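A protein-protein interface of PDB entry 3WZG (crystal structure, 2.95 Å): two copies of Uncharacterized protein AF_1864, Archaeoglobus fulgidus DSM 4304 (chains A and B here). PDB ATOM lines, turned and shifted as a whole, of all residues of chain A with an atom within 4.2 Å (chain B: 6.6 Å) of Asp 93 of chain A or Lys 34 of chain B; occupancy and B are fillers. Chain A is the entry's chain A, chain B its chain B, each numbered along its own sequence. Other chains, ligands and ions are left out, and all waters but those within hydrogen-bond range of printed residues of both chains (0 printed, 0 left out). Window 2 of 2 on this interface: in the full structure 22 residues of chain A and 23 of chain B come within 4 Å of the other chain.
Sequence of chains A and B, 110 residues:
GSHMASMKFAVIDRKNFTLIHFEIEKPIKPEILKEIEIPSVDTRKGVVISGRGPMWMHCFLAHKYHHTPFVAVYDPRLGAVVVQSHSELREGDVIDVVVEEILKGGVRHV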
ATOM      1  N   ALA A  80     -16.627 -32.822 -19.855  1.00  0.00           N
ATOM      2  CA  ALA A  80     -16.653 -33.307 -21.215  1.00  0.00           C
ATOM      3  C   ALA A  80     -17.873 -32.742 -21.868  1.00  0.00           C
ATOM      4  O   ALA A  80     -19.001 -32.991 -21.402  1.00  0.00           O
ATOM      5  CB  ALA A  80     -16.735 -34.814 -21.200  1.00  0.00           C
ATOM      6  N   VAL A  81     -17.661 -32.019 -22.956  1.00  0.00           N
ATOM      7  CA  VAL A  81     -18.739 -31.349 -23.660  1.00  0.00           C
ATOM      8  C   VAL A  81     -19.214 -32.186 -24.845  1.00  0.00           C
ATOM      9  O   VAL A  81     -18.429 -32.566 -25.719  1.00  0.00           O
ATOM     10  CB  VAL A  81     -18.235 -30.023 -24.217  1.00  0.00           C
ATOM     11  CG1 VAL A  81     -19.324 -29.298 -24.998  1.00  0.00           C
ATOM     12  CG2 VAL A  81     -17.684 -29.152 -23.103  1.00  0.00           C
ATOM     13  N   VAL A  82     -20.512 -32.438 -24.901  1.00  0.00           N
ATOM     14  CA  VAL A  82     -21.087 -33.214 -25.987  1.00  0.00           C
ATOM     15  C   VAL A  82     -21.144 -32.363 -27.210  1.00  0.00           C
ATOM     16  O   VAL A  82     -21.670 -31.273 -27.174  1.00  0.00           O
ATOM     17  CB  VAL A  82     -22.502 -33.665 -25.676  1.00  0.00           C
ATOM     18  CG1 VAL A  82     -23.082 -34.441 -26.863  1.00  0.00           C
ATOM     19  CG2 VAL A  82     -22.456 -34.528 -24.448  1.00  0.00           C
ATOM     20  N   LEU A  89     -27.555 -38.017 -25.049  1.00  0.00           N
ATOM     21  CA  LEU A  89     -27.407 -36.679 -24.541  1.00  0.00           C
ATOM     22  C   LEU A  89     -27.561 -35.680 -25.666  1.00  0.00           C
ATOM     23  O   LEU A  89     -27.722 -36.058 -26.788  1.00  0.00           O
ATOM     24  CB  LEU A  89     -26.023 -36.551 -23.949  1.00  0.00           C
ATOM     25  CG  LEU A  89     -25.706 -37.381 -22.699  1.00  0.00           C
ATOM     26  CD1 LEU A  89     -24.220 -37.482 -22.466  1.00  0.00           C
ATOM     27  CD2 LEU A  89     -26.291 -36.713 -21.484  1.00  0.00           C
ATOM     28  N   ARG A  90     -27.522 -34.396 -25.360  1.00  0.00           N
ATOM     29  CA  ARG A  90     -27.696 -33.371 -26.379  1.00  0.00           C
ATOM     30  C   ARG A  90     -26.421 -32.588 -26.599  1.00  0.00           C
ATOM     31  O   ARG A  90     -25.632 -32.377 -25.689  1.00  0.00           O
ATOM     32  CB  ARG A  90     -28.754 -32.371 -25.966  1.00  0.00           C
ATOM     33  CG  ARG A  90     -30.171 -32.739 -26.368  1.00  0.00           C
ATOM     34  CD  ARG A  90     -30.934 -31.485 -26.789  1.00  0.00           C
ATOM     35  NE  ARG A  90     -32.319 -31.542 -26.346  1.00  0.00           N
ATOM     36  CZ  ARG A  90     -32.895 -30.693 -25.502  1.00  0.00           C
ATOM     37  NH1 ARG A  90     -32.215 -29.677 -24.994  1.00  0.00           N
ATOM     38  NH2 ARG A  90     -34.175 -30.854 -25.176  1.00  0.00           N
ATOM     39  N   GLU A  91     -26.248 -32.116 -27.816  1.00  0.00           N
ATOM     40  CA  GLU A  91     -25.131 -31.290 -28.086  1.00  0.00           C
ATOM     41  C   GLU A  91     -25.102 -30.201 -27.068  1.00  0.00           C
ATOM     42  O   GLU A  91     -26.090 -29.607 -26.781  1.00  0.00           O
ATOM     43  CB  GLU A  91     -25.162 -30.768 -29.491  1.00  0.00           C
ATOM     44  CG  GLU A  91     -26.409 -30.019 -29.925  1.00  0.00           C
ATOM     45  CD  GLU A  91     -26.361 -29.778 -31.435  1.00  0.00           C
ATOM     46  OE1 GLU A  91     -25.478 -30.415 -32.136  1.00  0.00           O
ATOM     47  OE2 GLU A  91     -27.186 -28.958 -31.904  1.00  0.00           O
ATOM     48  N   GLY A  92     -23.954 -29.974 -26.472  1.00  0.00           N
ATOM     49  CA  GLY A  92     -23.796 -28.877 -25.509  1.00  0.00           C
ATOM     50  C   GLY A  92     -23.968 -29.283 -24.049  1.00  0.00           C
ATOM     51  O   GLY A  92     -23.521 -28.574 -23.152  1.00  0.00           O
ATOM     52  N   ASP A  93     -24.584 -30.433 -23.793  1.00  0.00           N
ATOM     53  CA  ASP A  93     -24.560 -30.997 -22.447  1.00  0.00           C
ATOM     54  C   ASP A  93     -23.143 -31.205 -21.944  1.00  0.00           C
ATOM     55  O   ASP A  93     -22.234 -31.357 -22.716  1.00  0.00           O
ATOM     56  CB  ASP A  93     -25.233 -32.354 -22.430  1.00  0.00           C
ATOM     57  CG  ASP A  93     -26.730 -32.271 -22.616  1.00  0.00           C
ATOM     58  OD1 ASP A  93     -27.277 -31.133 -22.708  1.00  0.00           O
ATOM     59  OD2 ASP A  93     -27.339 -33.375 -22.688  1.00  0.00           O
ATOM     60  N   VAL A  94     -22.964 -31.277 -20.635  1.00  0.00           N
ATOM     61  CA  VAL A  94     -21.657 -31.511 -20.093  1.00  0.00           C
ATOM     62  C   VAL A  94     -21.606 -32.687 -19.180  1.00  0.00           C
ATOM     63  O   VAL A  94     -22.281 -32.719 -18.191  1.00  0.00           O
ATOM     64  CB  VAL A  94     -21.180 -30.297 -19.302  1.00  0.00           C
ATOM     65  CG1 VAL A  94     -19.867 -30.625 -18.600  1.00  0.00           C
ATOM     66  CG2 VAL A  94     -21.001 -29.115 -20.249  1.00  0.00           C
ATOM     67  N   PRO B  30     -20.939 -24.002 -22.878  1.00  0.00           N
ATOM     68  CA  PRO B  30     -21.333 -25.050 -23.810  1.00  0.00           C
ATOM     69  C   PRO B  30     -22.824 -25.115 -24.151  1.00  0.00           C
ATOM     70  O   PRO B  30     -23.173 -25.722 -25.160  1.00  0.00           O
ATOM     71  CB  PRO B  30     -20.942 -26.336 -23.092  1.00  0.00           C
ATOM     72  CG  PRO B  30     -20.553 -25.959 -21.725  1.00  0.00           C
ATOM     73  CD  PRO B  30     -20.120 -24.535 -21.795  1.00  0.00           C
ATOM     74  N   GLU B  31     -23.690 -24.508 -23.346  1.00  0.00           N
ATOM     75  CA  GLU B  31     -25.092 -24.432 -23.697  1.00  0.00           C
ATOM     76  C   GLU B  31     -25.183 -23.781 -25.064  1.00  0.00           C
ATOM     77  O   GLU B  31     -26.098 -24.058 -25.843  1.00  0.00           O
ATOM     78  CB  GLU B  31     -25.863 -23.630 -22.664  1.00  0.00           C
ATOM     79  CG  GLU B  31     -27.327 -23.554 -22.950  1.00  0.00           C
ATOM     80  CD  GLU B  31     -27.684 -22.330 -23.770  1.00  0.00           C
ATOM     81  OE1 GLU B  31     -27.586 -22.328 -25.010  1.00  0.00           O
ATOM     82  OE2 GLU B  31     -28.073 -21.335 -23.158  1.00  0.00           O
ATOM     83  N   ILE B  32     -24.203 -22.979 -25.435  1.00  0.00           N
ATOM     84  CA  ILE B  32     -24.399 -22.227 -26.647  1.00  0.00           C
ATOM     85  C   ILE B  32     -24.534 -23.097 -27.877  1.00  0.00           C
ATOM     86  O   ILE B  32     -25.112 -22.691 -28.859  1.00  0.00           O
ATOM     87  CB  ILE B  32     -23.293 -21.197 -26.852  1.00  0.00           C
ATOM     88  CG1 ILE B  32     -23.769 -20.128 -27.848  1.00  0.00           C
ATOM     89  CG2 ILE B  32     -21.994 -21.856 -27.265  1.00  0.00           C
ATOM     90  CD1 ILE B  32     -22.727 -19.080 -28.158  1.00  0.00           C
ATOM     91  N   LEU B  33     -23.975 -24.296 -27.827  1.00  0.00           N
ATOM     92  CA  LEU B  33     -24.095 -25.245 -28.923  1.00  0.00           C
ATOM     93  C   LEU B  33     -25.541 -25.621 -29.252  1.00  0.00           C
ATOM     94  O   LEU B  33     -25.803 -26.161 -30.330  1.00  0.00           O
ATOM     95  CB  LEU B  33     -23.328 -26.522 -28.602  1.00  0.00           C
ATOM     96  CG  LEU B  33     -21.852 -26.399 -28.253  1.00  0.00           C
ATOM     97  CD1 LEU B  33     -21.289 -27.790 -28.103  1.00  0.00           C
ATOM     98  CD2 LEU B  33     -21.049 -25.631 -29.299  1.00  0.00           C
ATOM     99  N   LYS B  34     -26.465 -25.377 -28.327  1.00  0.00           N
ATOM    100  CA  LYS B  34     -27.878 -25.655 -28.585  1.00  0.00           C
ATOM    101  C   LYS B  34     -28.517 -24.565 -29.389  1.00  0.00           C
ATOM    102  O   LYS B  34     -29.487 -24.817 -30.060  1.00  0.00           O
ATOM    103  CB  LYS B  34     -28.636 -25.843 -27.282  1.00  0.00           C
ATOM    104  CG  LYS B  34     -28.045 -26.962 -26.464  1.00  0.00           C
ATOM    105  CD  LYS B  34     -28.907 -27.452 -25.323  1.00  0.00           C
ATOM    106  CE  LYS B  34     -28.348 -28.832 -25.006  1.00  0.00           C
ATOM    107  NZ  LYS B  34     -28.186 -29.230 -23.598  1.00  0.00           N
ATOM    108  N   GLU B  35     -27.937 -23.372 -29.333  1.00  0.00           N
ATOM    109  CA  GLU B  35     -28.499 -22.164 -29.927  1.00  0.00           C
ATOM    110  C   GLU B  35     -27.844 -21.803 -31.230  1.00  0.00           C
ATOM    111  O   GLU B  35     -28.438 -21.210 -32.117  1.00  0.00           O
ATOM    112  CB  GLU B  35     -28.273 -20.992 -28.980  1.00  0.00           C
ATOM    113  CG  GLU B  35     -29.184 -20.977 -27.759  1.00  0.00           C
ATOM    114  CD  GLU B  35     -28.870 -19.819 -26.819  1.00  0.00           C
ATOM    115  OE1 GLU B  35     -27.768 -19.225 -26.914  1.00  0.00           O
ATOM    116  OE2 GLU B  35     -29.749 -19.488 -25.996  1.00  0.00           O
ATOM    117  N   ILE B  36     -26.581 -22.114 -31.340  1.00  0.00           N
ATOM    118  CA  ILE B  36     -25.852 -21.671 -32.504  1.00  0.00           C
ATOM    119  C   ILE B  36     -26.563 -22.013 -33.798  1.00  0.00           C
ATOM    120  O   ILE B  36     -27.051 -23.123 -33.978  1.00  0.00           O
ATOM    121  CB  ILE B  36     -24.433 -22.257 -32.576  1.00  0.00           C
ATOM    122  CG1 ILE B  36     -23.495 -21.306 -31.900  1.00  0.00           C
ATOM    123  CG2 ILE B  36     -23.918 -22.385 -34.006  1.00  0.00           C
ATOM    124  CD1 ILE B  36     -22.103 -21.858 -31.823  1.00  0.00           C
ATOM    125  N   PHE B  60     -17.450 -29.359 -32.781  1.00  0.00           N
ATOM    126  CA  PHE B  60     -18.850 -29.192 -33.026  1.00  0.00           C
ATOM    127  C   PHE B  60     -19.033 -28.739 -34.444  1.00  0.00           C
ATOM    128  O   PHE B  60     -19.831 -29.313 -35.197  1.00  0.00           O
ATOM    129  CB  PHE B  60     -19.401 -28.172 -32.060  1.00  0.00           C
ATOM    130  CG  PHE B  60     -20.747 -27.677 -32.403  1.00  0.00           C
ATOM    131  CD1 PHE B  60     -21.875 -28.393 -32.061  1.00  0.00           C
ATOM    132  CD2 PHE B  60     -20.900 -26.453 -33.034  1.00  0.00           C
ATOM    133  CE1 PHE B  60     -23.147 -27.893 -32.340  1.00  0.00           C
ATOM    134  CE2 PHE B  60     -22.156 -25.954 -33.332  1.00  0.00           C
ATOM    135  CZ  PHE B  60     -23.276 -26.674 -32.979  1.00  0.00           C
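No position is printed for both chains.
OE2 of Glu 91 of chain A sits close to O of Leu 33 of chain B (3.5 Å).
OD1 of Asp 93 of chain A lies close to NZ of Lys 34 of chain B, at 2.3 Å.
Of the 8 printed residues of chain B, 4 touch a printed residue of chain A.
Printed residues of chain B that touch a printed residue of chain A: Pro 30, Leu 33, Lys 34 and Phe 60.
Along chain A the printed residues that touch a printed residue of chain B span positions 81 to 94.
Among the printed residues, 11 pairs touch across the chains.
Among the printed residues, Asp or Glu carboxylates within 4 Å of a Lys or Arg side-chain nitrogen of the other chain: Asp 93 of chain A with Lys 34 of chain B (2.3 Å).
The backbone carbonyl oxygen of Val 82 of chain A lies within hydrogen-bond range of the backbone NH of Gly 92 of chain A (2.7 Å).
The backbone NH (N) of Val 82 of chain A sits at hydrogen-bond distance from the backbone carbonyl oxygen (O) of Asp 93 of chain A.
The side-chain carboxylate of Asp 93 of chain A lies within hydrogen-bond range of the backbone NH of Arg 90 of chain A (2.9 Å).
Ala 80 of chain A touches none of the printed residues of chain B.
Of the printed residues of chain B, Val 81 of chain A touches Pro 30 and Leu 33.
Of the printed residues of chain B, Glu 91 of chain A touches Leu 33 (3.5 Å), Lys 34 (3.0 Å) and Phe 60 (3.4 Å).
Of the printed residues of chain A, Pro 30 of chain B touches Val 81 (3.9 Å), Gly 92 (3.2 Å) and Val 94 (3.5 Å).
Ile 32 of chain B touches none of the printed residues of chain A.
Of the printed residues of chain A, Leu 33 of chain B touches Val 81 (3.97 Å), Val 82 (3.6 Å), Glu 91 (3.5 Å) and Gly 92 (3.8 Å).
Lys 34 of chain B touches three residues of chain A.
The nearest printed residue of chain A that does not touch Phe 60 of chain B is Val 82 of chain A (5.7 Å).
Val 81 of chain A touches Pro 30 of chain B (CG1 to CB, 3.9 Å).
Leu 33 of chain B touches Val 81 of chain A.
Val 82 of chain A touches Leu 33 of chain B (O to CD1, 3.6 Å).
Lys 34 of chain B touches Arg 90 of chain A.
O of Glu 91 of chain A touches CE of Lys 34 of chain B (3.0 Å).
Glu 91 of chain A touches Phe 60 of chain B.
CA of Gly 92 of chain A touches O of Pro 30 of chain B, at 3.2 Å.
Leu 33 of chain B touches Gly 92 of chain A.
Val 94 of chain A touches Pro 30 of chain B.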
